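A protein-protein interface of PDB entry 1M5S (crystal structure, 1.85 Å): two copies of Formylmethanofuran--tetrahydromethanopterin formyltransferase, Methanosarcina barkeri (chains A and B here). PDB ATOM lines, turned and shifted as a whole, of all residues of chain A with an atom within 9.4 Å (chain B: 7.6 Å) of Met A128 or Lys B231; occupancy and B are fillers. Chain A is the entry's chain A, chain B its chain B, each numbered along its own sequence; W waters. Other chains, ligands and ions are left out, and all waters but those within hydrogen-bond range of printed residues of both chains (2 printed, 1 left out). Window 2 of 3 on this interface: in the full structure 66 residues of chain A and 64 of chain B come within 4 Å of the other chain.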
ATOM      1  N   LYS A 122       2.058 -10.478  -1.605  1.00  0.00           N
ATOM      2  CA  LYS A 122       1.554 -11.647  -0.883  1.00  0.00           C
ATOM      3  C   LYS A 122       0.231 -11.362  -0.176  1.00  0.00           C
ATOM      4  O   LYS A 122      -0.618 -12.245  -0.078  1.00  0.00           O
ATOM      5  CB  LYS A 122       2.591 -12.161   0.131  1.00  0.00           C
ATOM      6  CG  LYS A 122       2.619 -11.408   1.461  1.00  0.00           C
ATOM      7  CD  LYS A 122       3.529 -12.082   2.469  1.00  0.00           C
ATOM      8  CE  LYS A 122       3.592 -11.305   3.773  1.00  0.00           C
ATOM      9  NZ  LYS A 122       2.248 -11.027   4.352  1.00  0.00           N
ATOM     10  N   PHE A 123      -0.014 -10.087   0.110  1.00  0.00           N
ATOM     11  CA  PHE A 123      -1.223  -9.660   0.843  1.00  0.00           C
ATOM     12  C   PHE A 123      -2.496  -9.950   0.044  1.00  0.00           C
ATOM     13  O   PHE A 123      -3.608  -9.960   0.591  1.00  0.00           O
ATOM     14  CB  PHE A 123      -1.141  -8.174   1.158  1.00  0.00           C
ATOM     15  CG  PHE A 123      -0.185  -7.916   2.310  1.00  0.00           C
ATOM     16  CD1 PHE A 123       1.180  -7.776   2.055  1.00  0.00           C
ATOM     17  CD2 PHE A 123      -0.675  -7.841   3.616  1.00  0.00           C
ATOM     18  CE1 PHE A 123       2.067  -7.571   3.114  1.00  0.00           C
ATOM     19  CE2 PHE A 123       0.212  -7.641   4.678  1.00  0.00           C
ATOM     20  CZ  PHE A 123       1.584  -7.507   4.427  1.00  0.00           C
ATOM     21  N   PHE A 124      -2.324 -10.162  -1.261  1.00  0.00           N
ATOM     22  CA  PHE A 124      -3.440 -10.490  -2.133  1.00  0.00           C
ATOM     23  C   PHE A 124      -4.106 -11.814  -1.729  1.00  0.00           C
ATOM     24  O   PHE A 124      -5.304 -11.989  -1.922  1.00  0.00           O
ATOM     25  CB  PHE A 124      -2.974 -10.546  -3.593  1.00  0.00           C
ATOM     26  CG  PHE A 124      -4.092 -10.749  -4.580  1.00  0.00           C
ATOM     27  CD1 PHE A 124      -5.056  -9.767  -4.767  1.00  0.00           C
ATOM     28  CD2 PHE A 124      -4.189 -11.929  -5.310  1.00  0.00           C
ATOM     29  CE1 PHE A 124      -6.105  -9.954  -5.677  1.00  0.00           C
ATOM     30  CE2 PHE A 124      -5.233 -12.125  -6.219  1.00  0.00           C
ATOM     31  CZ  PHE A 124      -6.190 -11.140  -6.404  1.00  0.00           C
ATOM     32  N   ALA A 125      -3.339 -12.704  -1.106  1.00  0.00           N
ATOM     33  CA  ALA A 125      -3.834 -14.026  -0.736  1.00  0.00           C
ATOM     34  C   ALA A 125      -4.726 -13.995   0.505  1.00  0.00           C
ATOM     35  O   ALA A 125      -5.360 -15.002   0.842  1.00  0.00           O
ATOM     36  CB  ALA A 125      -2.667 -14.982  -0.525  1.00  0.00           C
ATOM     37  N   ASP A 126      -4.682 -12.883   1.240  1.00  0.00           N
ATOM     38  CA  ASP A 126      -5.668 -12.595   2.284  1.00  0.00           C
ATOM     39  C   ASP A 126      -5.628 -13.599   3.449  1.00  0.00           C
ATOM     40  O   ASP A 126      -6.663 -14.018   3.965  1.00  0.00           O
ATOM     41  CB  ASP A 126      -7.064 -12.553   1.652  1.00  0.00           C
ATOM     42  CG  ASP A 126      -8.121 -11.981   2.579  1.00  0.00           C
ATOM     43  OD1 ASP A 126      -7.783 -11.223   3.518  1.00  0.00           O
ATOM     44  OD2 ASP A 126      -9.305 -12.284   2.346  1.00  0.00           O
ATOM     45  N   GLY A 127      -4.421 -13.950   3.880  1.00  0.00           N
ATOM     46  CA  GLY A 127      -4.266 -14.927   4.938  1.00  0.00           C
ATOM     47  C   GLY A 127      -3.747 -16.267   4.451  1.00  0.00           C
ATOM     48  O   GLY A 127      -3.211 -17.046   5.242  1.00  0.00           O
ATOM     49  N   MET A 128      -3.867 -16.526   3.151  1.00  0.00           N
ATOM     50  CA  MET A 128      -3.524 -17.839   2.604  1.00  0.00           C
ATOM     51  C   MET A 128      -2.097 -17.932   2.054  1.00  0.00           C
ATOM     52  O   MET A 128      -1.663 -19.012   1.630  1.00  0.00           O
ATOM     53  CB  MET A 128      -4.523 -18.241   1.513  1.00  0.00           C
ATOM     54  CG  MET A 128      -5.985 -18.264   1.953  1.00  0.00           C
ATOM     55  SD  MET A 128      -6.335 -19.182   3.481  1.00  0.00           S
ATOM     56  CE  MET A 128      -5.730 -20.828   3.103  1.00  0.00           C
ATOM     57  N   GLU A 129      -1.350 -16.825   2.127  1.00  0.00           N
ATOM     58  CA  GLU A 129       0.041 -16.801   1.677  1.00  0.00           C
ATOM     59  C   GLU A 129       0.914 -17.771   2.449  1.00  0.00           C
ATOM     60  O   GLU A 129       0.714 -17.999   3.641  1.00  0.00           O
ATOM     61  CB  GLU A 129       0.656 -15.411   1.824  1.00  0.00           C
ATOM     62  CG  GLU A 129      -0.332 -14.285   1.870  1.00  0.00           C
ATOM     63  CD  GLU A 129      -0.587 -13.779   3.265  1.00  0.00           C
ATOM     64  OE1 GLU A 129       0.378 -13.556   4.024  1.00  0.00           O
ATOM     65  OE2 GLU A 129      -1.766 -13.558   3.582  1.00  0.00           O
ATOM     66  N   SER A 130       1.950 -18.252   1.776  1.00  0.00           N
ATOM     67  CA  SER A 130       2.956 -19.104   2.388  1.00  0.00           C
ATOM     68  C   SER A 130       4.313 -18.530   2.016  1.00  0.00           C
ATOM     69  O   SER A 130       4.415 -17.621   1.191  1.00  0.00           O
ATOM     70  CB  SER A 130       2.852 -20.546   1.862  1.00  0.00           C
ATOM     71  OG  SER A 130       1.706 -20.727   1.041  1.00  0.00           O
ATOM     72  N   GLU A 131       5.359 -19.097   2.598  1.00  0.00           N
ATOM     73  CA  GLU A 131       6.710 -18.688   2.284  1.00  0.00           C
ATOM     74  C   GLU A 131       7.526 -19.933   1.989  1.00  0.00           C
ATOM     75  O   GLU A 131       7.456 -20.920   2.720  1.00  0.00           O
ATOM     76  CB  GLU A 131       7.302 -17.928   3.465  1.00  0.00           C
ATOM     77  CG  GLU A 131       8.573 -17.184   3.144  1.00  0.00           C
ATOM     78  CD  GLU A 131       9.346 -16.825   4.389  1.00  0.00           C
ATOM     79  OE1 GLU A 131      10.531 -17.211   4.479  1.00  0.00           O
ATOM     80  OE2 GLU A 131       8.756 -16.189   5.290  1.00  0.00           O
ATOM     81  N   TYR A 140       7.486 -15.957  -1.943  1.00  0.00           N
ATOM     82  CA  TYR A 140       6.141 -15.963  -1.356  1.00  0.00           C
ATOM     83  C   TYR A 140       5.176 -16.668  -2.299  1.00  0.00           C
ATOM     84  O   TYR A 140       5.205 -16.451  -3.519  1.00  0.00           O
ATOM     85  CB  TYR A 140       5.652 -14.535  -1.119  1.00  0.00           C
ATOM     86  CG  TYR A 140       6.381 -13.872   0.038  1.00  0.00           C
ATOM     87  CD1 TYR A 140       6.044 -14.203   1.354  1.00  0.00           C
ATOM     88  CD2 TYR A 140       7.387 -12.942  -0.225  1.00  0.00           C
ATOM     89  CE1 TYR A 140       6.737 -13.616   2.416  1.00  0.00           C
ATOM     90  CE2 TYR A 140       8.085 -12.358   0.837  1.00  0.00           C
ATOM     91  CZ  TYR A 140       7.763 -12.699   2.157  1.00  0.00           C
ATOM     92  OH  TYR A 140       8.451 -12.141   3.187  1.00  0.00           O
ATOM     93  N   LYS A 141       4.400 -17.591  -1.733  1.00  0.00           N
ATOM     94  CA  LYS A 141       3.339 -18.288  -2.456  1.00  0.00           C
ATOM     95  C   LYS A 141       2.020 -17.554  -2.246  1.00  0.00           C
ATOM     96  O   LYS A 141       1.570 -17.390  -1.113  1.00  0.00           O
ATOM     97  CB  LYS A 141       3.207 -19.722  -1.935  1.00  0.00           C
ATOM     98  CG  LYS A 141       3.874 -20.773  -2.782  1.00  0.00           C
ATOM     99  CD  LYS A 141       3.283 -22.147  -2.488  1.00  0.00           C
ATOM    100  CE  LYS A 141       4.366 -23.151  -2.135  1.00  0.00           C
ATOM    101  NZ  LYS A 141       3.768 -24.423  -1.641  1.00  0.00           N
ATOM    102  N   VAL A 142       1.372 -17.183  -3.345  1.00  0.00           N
ATOM    103  CA  VAL A 142       0.074 -16.526  -3.305  1.00  0.00           C
ATOM    104  C   VAL A 142      -0.941 -17.398  -4.060  1.00  0.00           C
ATOM    105  O   VAL A 142      -0.960 -17.421  -5.294  1.00  0.00           O
ATOM    106  CB  VAL A 142       0.147 -15.105  -3.954  1.00  0.00           C
ATOM    107  CG1 VAL A 142      -1.204 -14.410  -3.874  1.00  0.00           C
ATOM    108  CG2 VAL A 142       1.226 -14.277  -3.275  1.00  0.00           C
ATOM    109  N   PRO A 143      -1.753 -18.184  -3.322  1.00  0.00           N
ATOM    110  CA  PRO A 143      -2.801 -18.993  -3.950  1.00  0.00           C
ATOM    111  C   PRO A 143      -3.777 -18.179  -4.797  1.00  0.00           C
ATOM    112  O   PRO A 143      -4.357 -17.196  -4.335  1.00  0.00           O
ATOM    113  CB  PRO A 143      -3.490 -19.658  -2.761  1.00  0.00           C
ATOM    114  CG  PRO A 143      -2.400 -19.802  -1.759  1.00  0.00           C
ATOM    115  CD  PRO A 143      -1.593 -18.530  -1.897  1.00  0.00           C
ATOM    116  N   ILE A 144      -3.872 -18.543  -6.070  1.00  0.00           N
ATOM    117  CA  ILE A 144      -4.824 -17.932  -6.992  1.00  0.00           C
ATOM    118  C   ILE A 144      -5.515 -19.025  -7.824  1.00  0.00           C
ATOM    119  O   ILE A 144      -5.235 -20.212  -7.643  1.00  0.00           O
ATOM    120  CB  ILE A 144      -4.123 -16.891  -7.923  1.00  0.00           C
ATOM    121  CG1 ILE A 144      -2.924 -17.527  -8.641  1.00  0.00           C
ATOM    122  CG2 ILE A 144      -3.672 -15.673  -7.103  1.00  0.00           C
ATOM    123  CD1 ILE A 144      -2.297 -16.635  -9.693  1.00  0.00           C
ATOM    124  N   GLY A 147      -3.576 -21.743  -9.612  1.00  0.00           N
ATOM    125  CA  GLY A 147      -2.564 -22.429  -8.826  1.00  0.00           C
ATOM    126  C   GLY A 147      -1.908 -21.487  -7.833  1.00  0.00           C
ATOM    127  O   GLY A 147      -2.585 -20.655  -7.238  1.00  0.00           O
ATOM    128  N   ASP A 148      -0.607 -21.656  -7.613  1.00  0.00           N
ATOM    129  CA  ASP A 148       0.160 -20.778  -6.726  1.00  0.00           C
ATOM    130  C   ASP A 148       1.034 -19.827  -7.552  1.00  0.00           C
ATOM    131  O   ASP A 148       1.778 -20.265  -8.436  1.00  0.00           O
ATOM    132  CB  ASP A 148       1.060 -21.608  -5.801  1.00  0.00           C
ATOM    133  CG  ASP A 148       0.272 -22.458  -4.808  1.00  0.00           C
ATOM    134  OD1 ASP A 148      -0.700 -21.949  -4.209  1.00  0.00           O
ATOM    135  OD2 ASP A 148       0.693 -23.609  -4.547  1.00  0.00           O
ATOM    136  N   PHE A 149       0.891 -18.526  -7.312  1.00  0.00           N
ATOM    137  CA  PHE A 149       1.793 -17.541  -7.900  1.00  0.00           C
ATOM    138  C   PHE A 149       3.020 -17.371  -6.997  1.00  0.00           C
ATOM    139  O   PHE A 149       2.890 -17.177  -5.791  1.00  0.00           O
ATOM    140  CB  PHE A 149       1.070 -16.203  -8.082  1.00  0.00           C
ATOM    141  CG  PHE A 149       1.964 -15.076  -8.535  1.00  0.00           C
ATOM    142  CD1 PHE A 149       2.629 -15.142  -9.757  1.00  0.00           C
ATOM    143  CD2 PHE A 149       2.129 -13.939  -7.744  1.00  0.00           C
ATOM    144  CE1 PHE A 149       3.441 -14.096 -10.187  1.00  0.00           C
ATOM    145  CE2 PHE A 149       2.941 -12.881  -8.165  1.00  0.00           C
ATOM    146  CZ  PHE A 149       3.598 -12.962  -9.391  1.00  0.00           C
ATOM    147  N   LYS B 207     -12.027 -11.507  -5.150  1.00  0.00           N
ATOM    148  CA  LYS B 207     -13.260 -11.186  -4.423  1.00  0.00           C
ATOM    149  C   LYS B 207     -13.190  -9.752  -3.909  1.00  0.00           C
ATOM    150  O   LYS B 207     -12.095  -9.195  -3.774  1.00  0.00           O
ATOM    151  CB  LYS B 207     -13.473 -12.156  -3.251  1.00  0.00           C
ATOM    152  CG  LYS B 207     -12.476 -12.031  -2.104  1.00  0.00           C
ATOM    153  CD  LYS B 207     -12.902 -12.899  -0.930  1.00  0.00           C
ATOM    154  CE  LYS B 207     -12.028 -12.682   0.284  1.00  0.00           C
ATOM    155  NZ  LYS B 207     -10.669 -13.264   0.112  1.00  0.00           N
ATOM    156  N   ASN B 211     -10.956 -11.021   4.060  1.00  0.00           N
ATOM    157  CA  ASN B 211     -11.332 -11.674   5.313  1.00  0.00           C
ATOM    158  C   ASN B 211     -10.314 -11.314   6.392  1.00  0.00           C
ATOM    159  O   ASN B 211     -10.656 -11.212   7.572  1.00  0.00           O
ATOM    160  CB  ASN B 211     -11.352 -13.205   5.156  1.00  0.00           C
ATOM    161  CG  ASN B 211     -12.198 -13.678   3.981  1.00  0.00           C
ATOM    162  OD1 ASN B 211     -13.339 -13.248   3.796  1.00  0.00           O
ATOM    163  ND2 ASN B 211     -11.647 -14.599   3.200  1.00  0.00           N
ATOM    164  N   LYS B 212      -9.045 -11.258   5.996  1.00  0.00           N
ATOM    165  CA  LYS B 212      -7.952 -11.007   6.928  1.00  0.00           C
ATOM    166  C   LYS B 212      -7.455  -9.568   6.805  1.00  0.00           C
ATOM    167  O   LYS B 212      -7.354  -8.860   7.806  1.00  0.00           O
ATOM    168  CB  LYS B 212      -6.807 -11.998   6.679  1.00  0.00           C
ATOM    169  CG  LYS B 212      -5.530 -11.724   7.464  1.00  0.00           C
ATOM    170  CD  LYS B 212      -5.366 -12.663   8.650  1.00  0.00           C
ATOM    171  CE  LYS B 212      -3.998 -12.499   9.301  1.00  0.00           C
ATOM    172  NZ  LYS B 212      -2.906 -13.144   8.513  1.00  0.00           N
ATOM    173  N   TYR B 213      -7.240  -9.112   5.571  1.00  0.00           N
ATOM    174  CA  TYR B 213      -6.695  -7.775   5.318  1.00  0.00           C
ATOM    175  C   TYR B 213      -7.767  -6.823   4.811  1.00  0.00           C
ATOM    176  O   TYR B 213      -7.826  -6.529   3.618  1.00  0.00           O
ATOM    177  CB  TYR B 213      -5.564  -7.849   4.295  1.00  0.00           C
ATOM    178  CG  TYR B 213      -4.477  -8.819   4.666  1.00  0.00           C
ATOM    179  CD1 TYR B 213      -3.858  -8.758   5.918  1.00  0.00           C
ATOM    180  CD2 TYR B 213      -4.074  -9.811   3.776  1.00  0.00           C
ATOM    181  CE1 TYR B 213      -2.863  -9.665   6.275  1.00  0.00           C
ATOM    182  CE2 TYR B 213      -3.080 -10.724   4.121  1.00  0.00           C
ATOM    183  CZ  TYR B 213      -2.479 -10.650   5.371  1.00  0.00           C
ATOM    184  OH  TYR B 213      -1.496 -11.556   5.713  1.00  0.00           O
ATOM    185  N   ALA B 220      -7.518 -12.339  -3.529  1.00  0.00           N
ATOM    186  CA  ALA B 220      -7.785 -13.673  -4.071  1.00  0.00           C
ATOM    187  C   ALA B 220      -9.037 -14.292  -3.437  1.00  0.00           C
ATOM    188  O   ALA B 220      -9.218 -14.247  -2.218  1.00  0.00           O
ATOM    189  CB  ALA B 220      -6.581 -14.580  -3.843  1.00  0.00           C
ATOM    190  N   ASN B 221      -9.947 -14.754  -4.288  1.00  0.00           N
ATOM    191  CA  ASN B 221     -11.092 -15.551  -3.858  1.00  0.00           C
ATOM    192  C   ASN B 221     -10.634 -16.967  -3.494  1.00  0.00           C
ATOM    193  O   ASN B 221     -10.490 -17.837  -4.365  1.00  0.00           O
ATOM    194  CB  ASN B 221     -12.138 -15.609  -4.975  1.00  0.00           C
ATOM    195  CG  ASN B 221     -13.506 -16.028  -4.475  1.00  0.00           C
ATOM    196  OD1 ASN B 221     -14.523 -15.617  -5.021  1.00  0.00           O
ATOM    197  ND2 ASN B 221     -13.538 -16.876  -3.457  1.00  0.00           N
ATOM    198  N   GLU B 222     -10.457 -17.198  -2.195  1.00  0.00           N
ATOM    199  CA  GLU B 222     -10.003 -18.481  -1.666  1.00  0.00           C
ATOM    200  C   GLU B 222     -10.862 -19.676  -2.106  1.00  0.00           C
ATOM    201  O   GLU B 222     -10.380 -20.813  -2.110  1.00  0.00           O
ATOM    202  CB  GLU B 222      -9.931 -18.424  -0.130  1.00  0.00           C
ATOM    203  CG  GLU B 222     -11.277 -18.240   0.594  1.00  0.00           C
ATOM    204  CD  GLU B 222     -11.802 -16.803   0.570  1.00  0.00           C
ATOM    205  OE1 GLU B 222     -11.044 -15.882   0.213  1.00  0.00           O
ATOM    206  OE2 GLU B 222     -12.980 -16.593   0.919  1.00  0.00           O
ATOM    207  N   CYS B 225      -9.431 -21.202  -5.466  1.00  0.00           N
ATOM    208  CA  CYS B 225      -8.007 -21.509  -5.447  1.00  0.00           C
ATOM    209  C   CYS B 225      -7.805 -23.009  -5.234  1.00  0.00           C
ATOM    210  O   CYS B 225      -7.999 -23.512  -4.131  1.00  0.00           O
ATOM    211  CB  CYS B 225      -7.314 -20.727  -4.320  1.00  0.00           C
ATOM    212  SG  CYS B 225      -7.366 -18.910  -4.482  1.00  0.00           S
ATOM    213  N   PRO B 226      -7.396 -23.738  -6.288  1.00  0.00           N
ATOM    214  CA  PRO B 226      -7.190 -25.193  -6.256  1.00  0.00           C
ATOM    215  C   PRO B 226      -6.204 -25.684  -5.196  1.00  0.00           C
ATOM    216  O   PRO B 226      -6.429 -26.719  -4.564  1.00  0.00           O
ATOM    217  CB  PRO B 226      -6.680 -25.509  -7.659  1.00  0.00           C
ATOM    218  CG  PRO B 226      -7.254 -24.429  -8.499  1.00  0.00           C
ATOM    219  CD  PRO B 226      -7.203 -23.202  -7.645  1.00  0.00           C
ATOM    220  N   SER B 227      -5.111 -24.944  -5.012  1.00  0.00           N
ATOM    221  CA  SER B 227      -4.006 -25.385  -4.156  1.00  0.00           C
ATOM    222  C   SER B 227      -4.332 -25.414  -2.661  1.00  0.00           C
ATOM    223  O   SER B 227      -3.581 -25.988  -1.871  1.00  0.00           O
ATOM    224  CB  SER B 227      -2.783 -24.500  -4.382  1.00  0.00           C
ATOM    225  OG  SER B 227      -3.030 -23.192  -3.910  1.00  0.00           O
ATOM    226  N   ILE B 228      -5.410 -24.736  -2.273  1.00  0.00           N
ATOM    227  CA  ILE B 228      -5.818 -24.664  -0.873  1.00  0.00           C
ATOM    228  C   ILE B 228      -7.264 -25.132  -0.683  1.00  0.00           C
ATOM    229  O   ILE B 228      -7.871 -24.879   0.359  1.00  0.00           O
ATOM    230  CB  ILE B 228      -5.671 -23.218  -0.314  1.00  0.00           C
ATOM    231  CG1 ILE B 228      -6.485 -22.239  -1.155  1.00  0.00           C
ATOM    232  CG2 ILE B 228      -4.206 -22.799  -0.299  1.00  0.00           C
ATOM    233  CD1 ILE B 228      -6.597 -20.866  -0.550  1.00  0.00           C
ATOM    234  N   LYS B 229      -7.775 -25.900  -1.644  1.00  0.00           N
ATOM    235  CA  LYS B 229      -9.191 -26.251  -1.675  1.00  0.00           C
ATOM    236  C   LYS B 229      -9.633 -27.151  -0.523  1.00  0.00           C
ATOM    237  O   LYS B 229     -10.806 -27.152  -0.154  1.00  0.00           O
ATOM    238  CB  LYS B 229      -9.560 -26.895  -3.017  1.00  0.00           C
ATOM    239  CG  LYS B 229      -9.014 -28.298  -3.253  1.00  0.00           C
ATOM    240  CD  LYS B 229      -9.352 -28.764  -4.666  1.00  0.00           C
ATOM    241  CE  LYS B 229      -8.707 -30.104  -4.997  1.00  0.00           C
ATOM    242  NZ  LYS B 229      -8.990 -30.503  -6.412  1.00  0.00           N
ATOM    243  N   ASP B 230      -8.688 -27.874   0.076  1.00  0.00           N
ATOM    244  CA  ASP B 230      -8.992 -28.754   1.200  1.00  0.00           C
ATOM    245  C   ASP B 230      -9.016 -28.003   2.535  1.00  0.00           C
ATOM    246  O   ASP B 230      -9.600 -28.484   3.512  1.00  0.00           O
ATOM    247  CB  ASP B 230      -7.990 -29.915   1.248  1.00  0.00           C
ATOM    248  CG  ASP B 230      -8.128 -30.864   0.054  1.00  0.00           C
ATOM    249  OD1 ASP B 230      -9.270 -31.153  -0.371  1.00  0.00           O
ATOM    250  OD2 ASP B 230      -7.089 -31.323  -0.465  1.00  0.00           O
ATOM    251  N   LYS B 231      -8.484 -26.780   2.536  1.00  0.00           N
ATOM    252  CA  LYS B 231      -8.567 -25.884   3.693  1.00  0.00           C
ATOM    253  C   LYS B 231      -9.829 -25.010   3.665  1.00  0.00           C
ATOM    254  O   LYS B 231     -10.113 -24.289   4.625  1.00  0.00           O
ATOM    255  CB  LYS B 231      -7.344 -24.962   3.747  1.00  0.00           C
ATOM    256  CG  LYS B 231      -6.000 -25.643   3.551  1.00  0.00           C
ATOM    257  CD  LYS B 231      -4.861 -24.632   3.673  1.00  0.00           C
ATOM    258  CE  LYS B 231      -3.505 -25.258   3.368  1.00  0.00           C
ATOM    259  NZ  LYS B 231      -3.178 -26.379   4.295  1.00  0.00           N
ATOM    260  N   ILE B 232     -10.541 -25.023   2.540  1.00  0.00           N
ATOM    261  CA  ILE B 232     -11.626 -24.076   2.284  1.00  0.00           C
ATOM    262  C   ILE B 232     -12.929 -24.853   2.065  1.00  0.00           C
ATOM    263  O   ILE B 232     -13.213 -25.307   0.956  1.00  0.00           O
ATOM    264  CB  ILE B 232     -11.315 -23.217   1.020  1.00  0.00           C
ATOM    265  CG1 ILE B 232      -9.927 -22.580   1.138  1.00  0.00           C
ATOM    266  CG2 ILE B 232     -12.377 -22.140   0.818  1.00  0.00           C
ATOM    267  CD1 ILE B 232      -9.736 -21.706   2.370  1.00  0.00           C
ATOM    268  N   GLU B 233     -13.719 -25.017   3.123  1.00  0.00           N
ATOM    269  CA  GLU B 233     -14.770 -26.035   3.113  1.00  0.00           C
ATOM    270  C   GLU B 233     -16.021 -25.646   2.321  1.00  0.00           C
ATOM    271  O   GLU B 233     -16.908 -26.475   2.096  1.00  0.00           O
ATOM    272  CB  GLU B 233     -15.137 -26.446   4.548  1.00  0.00           C
ATOM    273  CG  GLU B 233     -14.719 -27.883   4.916  1.00  0.00           C
ATOM    274  CD  GLU B 233     -13.375 -27.972   5.641  1.00  0.00           C
ATOM    275  OE1 GLU B 233     -12.516 -27.077   5.463  1.00  0.00           O
ATOM    276  OE2 GLU B 233     -13.171 -28.963   6.378  1.00  0.00           O
ATOM    277  N   ASN B 234     -16.022 -24.426   1.795  1.00  0.00           N
ATOM    278  CA  ASN B 234     -17.053 -23.973   0.861  1.00  0.00           C
ATOM    279  C   ASN B 234     -16.462 -23.814  -0.552  1.00  0.00           C
ATOM    280  O   ASN B 234     -16.977 -23.046  -1.377  1.00  0.00           O
ATOM    281  CB  ASN B 234     -17.634 -22.641   1.343  1.00  0.00           C
ATOM    282  CG  ASN B 234     -16.552 -21.636   1.741  1.00  0.00           C
ATOM    283  OD1 ASN B 234     -15.465 -22.011   2.196  1.00  0.00           O
ATOM    284  ND2 ASN B 234     -16.859 -20.352   1.595  1.00  0.00           N
ATOM    285  N   THR B 235     -15.416 -24.590  -0.835  1.00  0.00           N
ATOM    286  CA  THR B 235     -14.663 -24.474  -2.081  1.00  0.00           C
ATOM    287  C   THR B 235     -15.497 -24.762  -3.329  1.00  0.00           C
ATOM    288  O   THR B 235     -16.443 -25.550  -3.297  1.00  0.00           O
ATOM    289  CB  THR B 235     -13.408 -25.400  -2.067  1.00  0.00           C
ATOM    290  OG1 THR B 235     -12.632 -25.179  -3.250  1.00  0.00           O
ATOM    291  CG2 THR B 235     -13.806 -26.869  -1.998  1.00  0.00           C
HETATM  292  O   HOH W   1      -8.859 -15.647   2.464  1.00  0.00           O
HETATM  293  O   HOH W   2      -4.649 -22.172  -5.627  1.00  0.00           O
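The backbone carbonyl oxygen (O) of Phe A124 lies within hydrogen-bond range of the backbone NH (N) of Ala B220 (2.8 Å). The side-chain carboxylate (OD2) of Asp A126 is in salt-bridge range of the side-chain amino group (NZ) of Lys B207. The backbone NH of Asn B211 sits at hydrogen-bond distance from the side-chain carboxylate of Asp A126. OD1 of Asp A126 is in hydrogen-bond range of N of Lys B212, 2.8 Å away. OD1 of Asp A126 is in hydrogen-bond range of N of Tyr B213, 3.0 Å away. OE2 of Glu A129 lies within hydrogen-bond range of OH of Tyr B213. O of Pro A143 lies within hydrogen-bond range of SG of Cys B225, at 3.5 Å. The side-chain carboxylate (OD1) of Asp A148 is in hydrogen-bond range of the side-chain hydroxyl (OG) of Ser B227 (2.7 Å).
The side-chain carboxylate of Glu A129 is in salt-bridge range of the side-chain amino group of Lys A122, 3.2 Å away. The backbone NH (N) of Gly A127 lies within hydrogen-bond range of the side-chain carboxylate (OE2) of Glu A129 (2.7 Å). NZ of Lys B207 lies within hydrogen-bond range of O of Ala B220 (2.9 Å). The side-chain amino group (NZ) of Lys B207 is in salt-bridge range of the side-chain carboxylate (OE1) of Glu B222, at 2.6 Å. The side-chain amide nitrogen (ND2) of Asn B211 lies within hydrogen-bond range of the side-chain carboxylate (OE1) of Glu B222 (3.3 Å). O of Asn B221 sits at hydrogen-bond distance from SG of Cys B225, at 3.3 Å.
Among the printed residues, merely in contact across the chains: Phe A123 with Tyr B213 (3.2 Å), Gly A127 with Tyr B213 (3.5 Å), Met A128 with Ile B228 (3.7 Å), Met A128 with Lys B231 (3.9 Å), Pro A143 with Ala B220 (3.5 Å), Pro A143 with Ser B227 (3.7 Å), Pro A143 with Ile B228 (3.8 Å), Ile A144 with Cys B225 (3.7 Å) and Ile A144 with Pro B226 (3.6 Å).
Of chain B, only Ile B228 (3.7 Å) and Lys B231 (3.9 Å) come within 4 Å of Met A128. Of chain A, only Met A128 comes within 4 Å of Lys B231. Of chain B, only Tyr B213 (3.5 Å) comes within 4 Å of Gly A127. No residue of chain A comes within 4 Å of Ile B232. Of the printed residues of chain A, Pro B226 touches Ile A144. Printed residues of chain A within 4 Å of Ala B220: Phe A124 and Pro A143. Printed residues of chain B within 4 Å of Asp A126: Lys B207 (2.8 Å), Asn B211 (2.7 Å), Lys B212 (2.8 Å) and Tyr B213 (3.0 Å). Of the printed residues of chain B, Glu A129 touches Tyr B213. Of the printed residues of chain B, Asp A148 touches Ser B227 (2.7 Å). Gly A147 touches none of the printed residues of chain B. The nearest residue of chain B that does not touch Met A128 is Ile B232 (4.2 Å). The nearest printed residue of chain A that does not touch Lys B212 is Gly A127 (4.2 Å).
Printed residues of chain B that touch a printed residue of chain A: Lys B207, Asn B211, Lys B212, Tyr B213, Ala B220, Cys B225, Pro B226, Ser B227, Ile B228 and Lys B231. Printed residues of chain A that touch a printed residue of chain B: Phe A123, Phe A124, Asp A126, Gly A127, Met A128, Glu A129, Pro A143, Ile A144 and Asp A148.
No position is printed for both chains.
Water W2 lies within hydrogen-bond range of OG of Ser B227, O of Ile A144 and O of Gly A147. Water W1 lies within hydrogen-bond range of ND2 of Asn B211, O of Asp A126 and OE1 of Glu B222.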
